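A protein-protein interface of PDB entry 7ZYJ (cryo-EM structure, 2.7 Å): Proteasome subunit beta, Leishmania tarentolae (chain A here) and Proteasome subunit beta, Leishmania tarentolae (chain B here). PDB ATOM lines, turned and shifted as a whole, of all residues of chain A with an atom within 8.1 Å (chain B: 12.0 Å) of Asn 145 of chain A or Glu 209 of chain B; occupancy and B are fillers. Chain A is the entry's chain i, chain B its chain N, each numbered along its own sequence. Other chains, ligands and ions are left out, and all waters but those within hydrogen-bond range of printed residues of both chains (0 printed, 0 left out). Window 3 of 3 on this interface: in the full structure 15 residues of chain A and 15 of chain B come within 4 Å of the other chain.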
ATOM      1  N   VAL A   7       7.670 -29.221  -0.234  1.00  0.00           N
ATOM      2  CA  VAL A   7       6.548 -29.838   0.462  1.00  0.00           C
ATOM      3  C   VAL A   7       5.466 -30.164  -0.557  1.00  0.00           C
ATOM      4  O   VAL A   7       5.026 -29.287  -1.309  1.00  0.00           O
ATOM      5  CB  VAL A   7       6.003 -28.914   1.564  1.00  0.00           C
ATOM      6  CG1 VAL A   7       4.708 -29.472   2.129  1.00  0.00           C
ATOM      7  CG2 VAL A   7       7.027 -28.736   2.663  1.00  0.00           C
ATOM      8  N   TYR A   8       5.036 -31.419  -0.586  1.00  0.00           N
ATOM      9  CA  TYR A   8       3.981 -31.859  -1.489  1.00  0.00           C
ATOM     10  C   TYR A   8       2.798 -32.385  -0.675  1.00  0.00           C
ATOM     11  O   TYR A   8       2.730 -32.205   0.543  1.00  0.00           O
ATOM     12  CB  TYR A   8       4.517 -32.885  -2.491  1.00  0.00           C
ATOM     13  CG  TYR A   8       4.752 -34.277  -1.950  1.00  0.00           C
ATOM     14  CD1 TYR A   8       5.901 -34.579  -1.233  1.00  0.00           C
ATOM     15  CD2 TYR A   8       3.840 -35.298  -2.181  1.00  0.00           C
ATOM     16  CE1 TYR A   8       6.125 -35.851  -0.749  1.00  0.00           C
ATOM     17  CE2 TYR A   8       4.054 -36.571  -1.699  1.00  0.00           C
ATOM     18  CZ  TYR A   8       5.199 -36.841  -0.984  1.00  0.00           C
ATOM     19  OH  TYR A   8       5.419 -38.109  -0.501  1.00  0.00           O
ATOM     20  N   ARG A   9       1.847 -33.009  -1.380  1.00  0.00           N
ATOM     21  CA  ARG A   9       0.579 -33.442  -0.796  1.00  0.00           C
ATOM     22  C   ARG A   9       0.744 -34.098   0.572  1.00  0.00           C
ATOM     23  O   ARG A   9       0.128 -33.673   1.555  1.00  0.00           O
ATOM     24  CB  ARG A   9      -0.120 -34.401  -1.761  1.00  0.00           C
ATOM     25  CG  ARG A   9      -1.507 -34.831  -1.332  1.00  0.00           C
ATOM     26  CD  ARG A   9      -2.253 -35.451  -2.499  1.00  0.00           C
ATOM     27  NE  ARG A   9      -2.245 -34.578  -3.667  1.00  0.00           N
ATOM     28  CZ  ARG A   9      -2.674 -34.933  -4.870  1.00  0.00           C
ATOM     29  NH1 ARG A   9      -3.152 -36.144  -5.105  1.00  0.00           N
ATOM     30  NH2 ARG A   9      -2.620 -34.050  -5.864  1.00  0.00           N
ATOM     31  N   ASP A  10       1.574 -35.138   0.655  1.00  0.00           N
ATOM     32  CA  ASP A  10       1.839 -35.821   1.926  1.00  0.00           C
ATOM     33  C   ASP A  10       3.309 -36.240   2.011  1.00  0.00           C
ATOM     34  O   ASP A  10       3.691 -37.346   1.627  1.00  0.00           O
ATOM     35  CB  ASP A  10       0.869 -36.988   2.114  1.00  0.00           C
ATOM     36  CG  ASP A  10       0.786 -37.915   0.899  1.00  0.00           C
ATOM     37  OD1 ASP A  10       1.802 -38.195   0.237  1.00  0.00           O
ATOM     38  OD2 ASP A  10      -0.341 -38.353   0.587  1.00  0.00           O
ATOM     39  N   PRO A 108       3.993 -32.599   7.292  1.00  0.00           N
ATOM     40  CA  PRO A 108       5.318 -32.299   6.736  1.00  0.00           C
ATOM     41  C   PRO A 108       5.889 -31.001   7.290  1.00  0.00           C
ATOM     42  O   PRO A 108       5.168 -30.040   7.561  1.00  0.00           O
ATOM     43  CB  PRO A 108       5.060 -32.196   5.227  1.00  0.00           C
ATOM     44  CG  PRO A 108       3.577 -32.085   5.078  1.00  0.00           C
ATOM     45  CD  PRO A 108       2.981 -32.793   6.243  1.00  0.00           C
ATOM     46  N   LEU A 122       9.333 -22.941   5.120  1.00  0.00           N
ATOM     47  CA  LEU A 122       8.737 -22.552   3.853  1.00  0.00           C
ATOM     48  C   LEU A 122       8.297 -23.794   3.095  1.00  0.00           C
ATOM     49  O   LEU A 122       8.790 -24.896   3.359  1.00  0.00           O
ATOM     50  CB  LEU A 122       9.726 -21.738   3.006  1.00  0.00           C
ATOM     51  CG  LEU A 122      10.039 -20.335   3.522  1.00  0.00           C
ATOM     52  CD1 LEU A 122      11.411 -19.884   3.051  1.00  0.00           C
ATOM     53  CD2 LEU A 122       8.960 -19.358   3.086  1.00  0.00           C
ATOM     54  N   PRO A 123       7.359 -23.651   2.144  1.00  0.00           N
ATOM     55  CA  PRO A 123       6.911 -24.816   1.368  1.00  0.00           C
ATOM     56  C   PRO A 123       7.962 -25.330   0.398  1.00  0.00           C
ATOM     57  O   PRO A 123       8.008 -26.527   0.100  1.00  0.00           O
ATOM     58  CB  PRO A 123       5.675 -24.294   0.620  1.00  0.00           C
ATOM     59  CG  PRO A 123       5.348 -22.978   1.233  1.00  0.00           C
ATOM     60  CD  PRO A 123       6.612 -22.434   1.784  1.00  0.00           C
ATOM     61  N   TYR A 142       6.165 -24.460  -9.008  1.00  0.00           N
ATOM     62  CA  TYR A 142       5.632 -25.003  -7.766  1.00  0.00           C
ATOM     63  C   TYR A 142       4.146 -24.701  -7.649  1.00  0.00           C
ATOM     64  O   TYR A 142       3.696 -23.599  -7.977  1.00  0.00           O
ATOM     65  CB  TYR A 142       6.375 -24.431  -6.559  1.00  0.00           C
ATOM     66  CG  TYR A 142       5.793 -24.862  -5.233  1.00  0.00           C
ATOM     67  CD1 TYR A 142       6.114 -26.093  -4.681  1.00  0.00           C
ATOM     68  CD2 TYR A 142       4.916 -24.041  -4.535  1.00  0.00           C
ATOM     69  CE1 TYR A 142       5.582 -26.496  -3.474  1.00  0.00           C
ATOM     70  CE2 TYR A 142       4.379 -24.436  -3.326  1.00  0.00           C
ATOM     71  CZ  TYR A 142       4.716 -25.664  -2.802  1.00  0.00           C
ATOM     72  OH  TYR A 142       4.185 -26.064  -1.599  1.00  0.00           O
ATOM     73  N   LYS A 143       3.385 -25.684  -7.177  1.00  0.00           N
ATOM     74  CA  LYS A 143       1.985 -25.504  -6.835  1.00  0.00           C
ATOM     75  C   LYS A 143       1.677 -26.319  -5.588  1.00  0.00           C
ATOM     76  O   LYS A 143       2.387 -27.269  -5.250  1.00  0.00           O
ATOM     77  CB  LYS A 143       1.054 -25.913  -7.986  1.00  0.00           C
ATOM     78  CG  LYS A 143       1.200 -27.355  -8.424  1.00  0.00           C
ATOM     79  CD  LYS A 143      -0.039 -27.834  -9.159  1.00  0.00           C
ATOM     80  CE  LYS A 143       0.215 -29.150  -9.874  1.00  0.00           C
ATOM     81  NZ  LYS A 143       1.102 -28.978 -11.055  1.00  0.00           N
ATOM     82  N   ASP A 144       0.612 -25.930  -4.896  1.00  0.00           N
ATOM     83  CA  ASP A 144       0.236 -26.597  -3.660  1.00  0.00           C
ATOM     84  C   ASP A 144      -0.327 -27.987  -3.938  1.00  0.00           C
ATOM     85  O   ASP A 144      -0.988 -28.222  -4.954  1.00  0.00           O
ATOM     86  CB  ASP A 144      -0.791 -25.765  -2.893  1.00  0.00           C
ATOM     87  CG  ASP A 144      -0.147 -24.710  -2.018  1.00  0.00           C
ATOM     88  OD1 ASP A 144       1.092 -24.733  -1.872  1.00  0.00           O
ATOM     89  OD2 ASP A 144      -0.880 -23.857  -1.475  1.00  0.00           O
ATOM     90  N   ASN A 145      -0.045 -28.909  -3.017  1.00  0.00           N
ATOM     91  CA  ASN A 145      -0.602 -30.264  -3.037  1.00  0.00           C
ATOM     92  C   ASN A 145      -0.242 -31.012  -4.320  1.00  0.00           C
ATOM     93  O   ASN A 145      -1.102 -31.572  -5.002  1.00  0.00           O
ATOM     94  CB  ASN A 145      -2.119 -30.232  -2.831  1.00  0.00           C
ATOM     95  CG  ASN A 145      -2.510 -29.732  -1.456  1.00  0.00           C
ATOM     96  OD1 ASN A 145      -2.324 -30.423  -0.455  1.00  0.00           O
ATOM     97  ND2 ASN A 145      -3.056 -28.522  -1.401  1.00  0.00           N
ATOM     98  N   MET A 146       1.047 -31.021  -4.649  1.00  0.00           N
ATOM     99  CA  MET A 146       1.514 -31.838  -5.759  1.00  0.00           C
ATOM    100  C   MET A 146       1.577 -33.304  -5.354  1.00  0.00           C
ATOM    101  O   MET A 146       1.732 -33.642  -4.179  1.00  0.00           O
ATOM    102  CB  MET A 146       2.896 -31.387  -6.228  1.00  0.00           C
ATOM    103  CG  MET A 146       2.940 -30.014  -6.851  1.00  0.00           C
ATOM    104  SD  MET A 146       4.595 -29.608  -7.429  1.00  0.00           S
ATOM    105  CE  MET A 146       5.415 -29.296  -5.872  1.00  0.00           C
ATOM    106  N   THR A 147       1.464 -34.182  -6.346  1.00  0.00           N
ATOM    107  CA  THR A 147       1.681 -35.595  -6.095  1.00  0.00           C
ATOM    108  C   THR A 147       3.172 -35.868  -5.910  1.00  0.00           C
ATOM    109  O   THR A 147       4.021 -34.988  -6.075  1.00  0.00           O
ATOM    110  CB  THR A 147       1.121 -36.442  -7.235  1.00  0.00           C
ATOM    111  OG1 THR A 147       1.507 -35.875  -8.492  1.00  0.00           O
ATOM    112  CG2 THR A 147      -0.396 -36.501  -7.159  1.00  0.00           C
ATOM    113  N   CYS A 148       3.488 -37.113  -5.551  1.00  0.00           N
ATOM    114  CA  CYS A 148       4.882 -37.483  -5.332  1.00  0.00           C
ATOM    115  C   CYS A 148       5.696 -37.359  -6.615  1.00  0.00           C
ATOM    116  O   CYS A 148       6.833 -36.876  -6.590  1.00  0.00           O
ATOM    117  CB  CYS A 148       4.966 -38.904  -4.775  1.00  0.00           C
ATOM    118  SG  CYS A 148       6.627 -39.419  -4.288  1.00  0.00           S
ATOM    119  N   GLU A 150       5.125 -35.396  -9.272  1.00  0.00           N
ATOM    120  CA  GLU A 150       5.323 -33.995  -9.629  1.00  0.00           C
ATOM    121  C   GLU A 150       6.390 -33.350  -8.757  1.00  0.00           C
ATOM    122  O   GLU A 150       7.245 -32.610  -9.257  1.00  0.00           O
ATOM    123  CB  GLU A 150       4.007 -33.226  -9.515  1.00  0.00           C
ATOM    124  CG  GLU A 150       2.884 -33.776 -10.373  1.00  0.00           C
ATOM    125  CD  GLU A 150       1.589 -33.007 -10.197  1.00  0.00           C
ATOM    126  OE1 GLU A 150       1.158 -32.820  -9.038  1.00  0.00           O
ATOM    127  OE2 GLU A 150       1.000 -32.590 -11.215  1.00  0.00           O
ATOM    128  N   ALA A 151       6.358 -33.619  -7.450  1.00  0.00           N
ATOM    129  CA  ALA A 151       7.362 -33.053  -6.556  1.00  0.00           C
ATOM    130  C   ALA A 151       8.754 -33.578  -6.884  1.00  0.00           C
ATOM    131  O   ALA A 151       9.725 -32.814  -6.886  1.00  0.00           O
ATOM    132  CB  ALA A 151       7.001 -33.355  -5.104  1.00  0.00           C
ATOM    133  N   HIS B 205       1.531 -14.585  -7.438  1.00  0.00           N
ATOM    134  CA  HIS B 205       0.846 -15.487  -6.521  1.00  0.00           C
ATOM    135  C   HIS B 205       1.490 -15.371  -5.148  1.00  0.00           C
ATOM    136  O   HIS B 205       2.705 -15.545  -5.014  1.00  0.00           O
ATOM    137  CB  HIS B 205       0.901 -16.932  -7.022  1.00  0.00           C
ATOM    138  CG  HIS B 205       0.032 -17.872  -6.246  1.00  0.00           C
ATOM    139  ND1 HIS B 205       0.511 -18.649  -5.214  1.00  0.00           N
ATOM    140  CD2 HIS B 205      -1.287 -18.161  -6.354  1.00  0.00           C
ATOM    141  CE1 HIS B 205      -0.475 -19.377  -4.719  1.00  0.00           C
ATOM    142  NE2 HIS B 205      -1.577 -19.099  -5.393  1.00  0.00           N
ATOM    143  N   TRP B 206       0.674 -15.083  -4.132  1.00  0.00           N
ATOM    144  CA  TRP B 206       1.150 -14.944  -2.761  1.00  0.00           C
ATOM    145  C   TRP B 206       0.280 -15.717  -1.778  1.00  0.00           C
ATOM    146  O   TRP B 206       0.307 -15.430  -0.577  1.00  0.00           O
ATOM    147  CB  TRP B 206       1.204 -13.470  -2.352  1.00  0.00           C
ATOM    148  CG  TRP B 206       2.077 -12.619  -3.217  1.00  0.00           C
ATOM    149  CD1 TRP B 206       1.739 -12.042  -4.406  1.00  0.00           C
ATOM    150  CD2 TRP B 206       3.428 -12.227  -2.951  1.00  0.00           C
ATOM    151  NE1 TRP B 206       2.799 -11.326  -4.902  1.00  0.00           N
ATOM    152  CE2 TRP B 206       3.848 -11.424  -4.026  1.00  0.00           C
ATOM    153  CE3 TRP B 206       4.323 -12.485  -1.909  1.00  0.00           C
ATOM    154  CZ2 TRP B 206       5.125 -10.874  -4.090  1.00  0.00           C
ATOM    155  CZ3 TRP B 206       5.590 -11.939  -1.974  1.00  0.00           C
ATOM    156  CH2 TRP B 206       5.980 -11.143  -3.057  1.00  0.00           C
ATOM    157  N   GLU B 207      -0.494 -16.691  -2.257  1.00  0.00           N
ATOM    158  CA  GLU B 207      -1.501 -17.361  -1.443  1.00  0.00           C
ATOM    159  C   GLU B 207      -1.165 -18.830  -1.211  1.00  0.00           C
ATOM    160  O   GLU B 207      -2.062 -19.672  -1.135  1.00  0.00           O
ATOM    161  CB  GLU B 207      -2.882 -17.225  -2.084  1.00  0.00           C
ATOM    162  CG  GLU B 207      -3.294 -15.790  -2.377  1.00  0.00           C
ATOM    163  CD  GLU B 207      -3.792 -15.058  -1.147  1.00  0.00           C
ATOM    164  OE1 GLU B 207      -2.976 -14.777  -0.245  1.00  0.00           O
ATOM    165  OE2 GLU B 207      -5.004 -14.764  -1.083  1.00  0.00           O
ATOM    166  N   TYR B 208       0.120 -19.154  -1.104  1.00  0.00           N
ATOM    167  CA  TYR B 208       0.515 -20.513  -0.767  1.00  0.00           C
ATOM    168  C   TYR B 208       0.122 -20.835   0.668  1.00  0.00           C
ATOM    169  O   TYR B 208       0.211 -19.987   1.558  1.00  0.00           O
ATOM    170  CB  TYR B 208       2.021 -20.693  -0.958  1.00  0.00           C
ATOM    171  CG  TYR B 208       2.464 -20.614  -2.399  1.00  0.00           C
ATOM    172  CD1 TYR B 208       1.979 -21.508  -3.343  1.00  0.00           C
ATOM    173  CD2 TYR B 208       3.367 -19.646  -2.817  1.00  0.00           C
ATOM    174  CE1 TYR B 208       2.379 -21.442  -4.661  1.00  0.00           C
ATOM    175  CE2 TYR B 208       3.773 -19.572  -4.134  1.00  0.00           C
ATOM    176  CZ  TYR B 208       3.276 -20.473  -5.052  1.00  0.00           C
ATOM    177  OH  TYR B 208       3.676 -20.404  -6.365  1.00  0.00           O
ATOM    178  N   GLU B 209      -0.325 -22.075   0.888  1.00  0.00           N
ATOM    179  CA  GLU B 209      -0.772 -22.471   2.219  1.00  0.00           C
ATOM    180  C   GLU B 209       0.366 -22.438   3.231  1.00  0.00           C
ATOM    181  O   GLU B 209       0.123 -22.245   4.427  1.00  0.00           O
ATOM    182  CB  GLU B 209      -1.405 -23.862   2.172  1.00  0.00           C
ATOM    183  CG  GLU B 209      -0.477 -24.956   1.672  1.00  0.00           C
ATOM    184  CD  GLU B 209      -1.197 -26.272   1.443  1.00  0.00           C
ATOM    185  OE1 GLU B 209      -2.417 -26.337   1.698  1.00  0.00           O
ATOM    186  OE2 GLU B 209      -0.541 -27.240   1.007  1.00  0.00           O
ATOM    187  N   GLY B 210       1.603 -22.623   2.780  1.00  0.00           N
ATOM    188  CA  GLY B 210       2.753 -22.519   3.651  1.00  0.00           C
ATOM    189  C   GLY B 210       3.198 -21.112   3.962  1.00  0.00           C
ATOM    190  O   GLY B 210       4.121 -20.923   4.758  1.00  0.00           O
ATOM    191  N   TYR B 211       2.566 -20.113   3.352  1.00  0.00           N
ATOM    192  CA  TYR B 211       2.893 -18.713   3.579  1.00  0.00           C
ATOM    193  C   TYR B 211       2.074 -18.089   4.700  1.00  0.00           C
ATOM    194  O   TYR B 211       2.250 -16.901   4.986  1.00  0.00           O
ATOM    195  CB  TYR B 211       2.680 -17.905   2.295  1.00  0.00           C
ATOM    196  CG  TYR B 211       3.835 -17.958   1.321  1.00  0.00           C
ATOM    197  CD1 TYR B 211       4.857 -18.884   1.471  1.00  0.00           C
ATOM    198  CD2 TYR B 211       3.903 -17.076   0.250  1.00  0.00           C
ATOM    199  CE1 TYR B 211       5.913 -18.932   0.582  1.00  0.00           C
ATOM    200  CE2 TYR B 211       4.954 -17.116  -0.643  1.00  0.00           C
ATOM    201  CZ  TYR B 211       5.956 -18.046  -0.473  1.00  0.00           C
ATOM    202  OH  TYR B 211       7.005 -18.091  -1.360  1.00  0.00           O
ATOM    203  N   CYS B 212       1.191 -18.855   5.336  1.00  0.00           N
ATOM    204  CA  CYS B 212       0.266 -18.294   6.307  1.00  0.00           C
ATOM    205  C   CYS B 212       1.001 -17.851   7.571  1.00  0.00           C
ATOM    206  O   CYS B 212       2.174 -18.165   7.793  1.00  0.00           O
ATOM    207  CB  CYS B 212      -0.826 -19.305   6.653  1.00  0.00           C
ATOM    208  SG  CYS B 212      -0.218 -20.901   7.225  1.00  0.00           S
ATOM    209  N   PHE B 213       0.281 -17.100   8.406  1.00  0.00           N
ATOM    210  CA  PHE B 213       0.869 -16.532   9.613  1.00  0.00           C
ATOM    211  C   PHE B 213       1.314 -17.610  10.594  1.00  0.00           C
ATOM    212  O   PHE B 213       2.380 -17.485  11.206  1.00  0.00           O
ATOM    213  CB  PHE B 213      -0.134 -15.589  10.276  1.00  0.00           C
ATOM    214  CG  PHE B 213       0.478 -14.639  11.267  1.00  0.00           C
ATOM    215  CD1 PHE B 213       0.761 -15.048  12.559  1.00  0.00           C
ATOM    216  CD2 PHE B 213       0.762 -13.335  10.907  1.00  0.00           C
ATOM    217  CE1 PHE B 213       1.320 -14.175  13.471  1.00  0.00           C
ATOM    218  CE2 PHE B 213       1.321 -12.456  11.815  1.00  0.00           C
ATOM    219  CZ  PHE B 213       1.600 -12.878  13.099  1.00  0.00           C
ATOM    220  N   GLU B 214       0.520 -18.668  10.762  1.00  0.00           N
ATOM    221  CA  GLU B 214       0.824 -19.656  11.792  1.00  0.00           C
ATOM    222  C   GLU B 214       1.931 -20.619  11.376  1.00  0.00           C
ATOM    223  O   GLU B 214       2.706 -21.061  12.230  1.00  0.00           O
ATOM    224  CB  GLU B 214      -0.441 -20.428  12.178  1.00  0.00           C
ATOM    225  CG  GLU B 214      -0.990 -21.361  11.109  1.00  0.00           C
ATOM    226  CD  GLU B 214      -1.895 -20.654  10.116  1.00  0.00           C
ATOM    227  OE1 GLU B 214      -1.870 -19.406  10.061  1.00  0.00           O
ATOM    228  OE2 GLU B 214      -2.637 -21.349   9.389  1.00  0.00           O
ATOM    229  N   LYS B 215       2.030 -20.956  10.089  1.00  0.00           N
ATOM    230  CA  LYS B 215       3.082 -21.868   9.656  1.00  0.00           C
ATOM    231  C   LYS B 215       4.443 -21.188   9.590  1.00  0.00           C
ATOM    232  O   LYS B 215       5.468 -21.843   9.806  1.00  0.00           O
ATOM    233  CB  LYS B 215       2.736 -22.475   8.296  1.00  0.00           C
ATOM    234  CG  LYS B 215       2.005 -23.804   8.378  1.00  0.00           C
ATOM    235  CD  LYS B 215       1.772 -24.389   6.997  1.00  0.00           C
ATOM    236  CE  LYS B 215       0.751 -25.514   7.035  1.00  0.00           C
ATOM    237  NZ  LYS B 215       1.276 -26.720   7.734  1.00  0.00           N
ATOM    238  N   THR B 216       4.476 -19.892   9.296  1.00  0.00           N
ATOM    239  CA  THR B 216       5.722 -19.144   9.228  1.00  0.00           C
ATOM    240  C   THR B 216       6.105 -18.508  10.556  1.00  0.00           C
ATOM    241  O   THR B 216       7.173 -17.895  10.647  1.00  0.00           O
ATOM    242  CB  THR B 216       5.629 -18.056   8.152  1.00  0.00           C
ATOM    243  OG1 THR B 216       4.437 -17.287   8.353  1.00  0.00           O
ATOM    244  CG2 THR B 216       5.597 -18.678   6.767  1.00  0.00           C
ATOM    245  N   ALA B 217       5.269 -18.642  11.581  1.00  0.00           N
ATOM    246  CA  ALA B 217       5.548 -18.010  12.862  1.00  0.00           C
ATOM    247  C   ALA B 217       6.679 -18.726  13.588  1.00  0.00           C
ATOM    248  O   ALA B 217       6.834 -19.947  13.487  1.00  0.00           O
ATOM    249  CB  ALA B 217       4.295 -18.001  13.734  1.00  0.00           C
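OD2 of Asp 144 of chain A lies within hydrogen-bond range of N of Glu 209 of chain B, 3.0 Å away.
The backbone carbonyl oxygen (O) of Glu 209 of chain B is in hydrogen-bond range of the side-chain sulfur (SG) of Cys 212 of chain B (3.1 Å). The side-chain carboxylate of Asp 144 of chain A lies within hydrogen-bond range of the side-chain hydroxyl of Tyr 142 of chain A (3.4 Å). NH2 of Arg 9 of chain A lies within hydrogen-bond range of O of Asn 145 of chain A (3.0 Å). The backbone carbonyl oxygen (O) of Pro 123 of chain A is in hydrogen-bond range of the backbone NH (N) of Val 7 of chain A, at 2.7 Å. The backbone carbonyl oxygen of Val 7 of chain A sits at hydrogen-bond distance from the side-chain hydroxyl of Tyr 142 of chain A (3.3 Å).
Among the printed residues, merely in contact across the chains: Pro 123 of chain A with Gly 210 of chain B (3.6 Å), Tyr 142 of chain A with Tyr 208 of chain B (3.6 Å), Asp 144 of chain A with Tyr 208 of chain B (3.7 Å), Asn 145 of chain A with Glu 209 of chain B (3.7 Å), Pro 123 of chain A with Tyr 211 of chain B (3.8 Å) and Leu 122 of chain A with Tyr 211 of chain B (3.97 Å).
Asn 145 of chain A touches just one residue of chain B: Glu 209 (3.7 Å). Glu 209 of chain B touches just these residues of chain A: Asp 144 and Asn 145. Arg 9 of chain A touches none of the printed residues of chain B. Printed residues of chain B within 4 Å of Asp 144 of chain A: Tyr 208 and Glu 209. No residue of chain B comes within 4 Å of Thr 147 of chain A. Printed residues of chain A within 4 Å of Tyr 211 of chain B: Leu 122 (3.97 Å) and Pro 123 (3.8 Å). Of the printed residues of chain A, Tyr 208 of chain B touches Tyr 142 (3.6 Å) and Asp 144 (3.7 Å). Of the printed residues of chain B, Tyr 142 of chain A touches Tyr 208. Of the printed residues of chain B, Pro 123 of chain A touches Gly 210 and Tyr 211.
Hydrophobic or aromatic side chains of chain A that line the printed part of chain B: Leu 122, Pro 123 and Tyr 142. Hydrophobic or aromatic side chains of chain B within 4 Å of the printed part of chain A: Tyr 208 and Tyr 211. Along chain B the printed residues that touch a printed residue of chain A span positions 208 to 211. Among the printed residues, 7 pairs touch across the chains.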
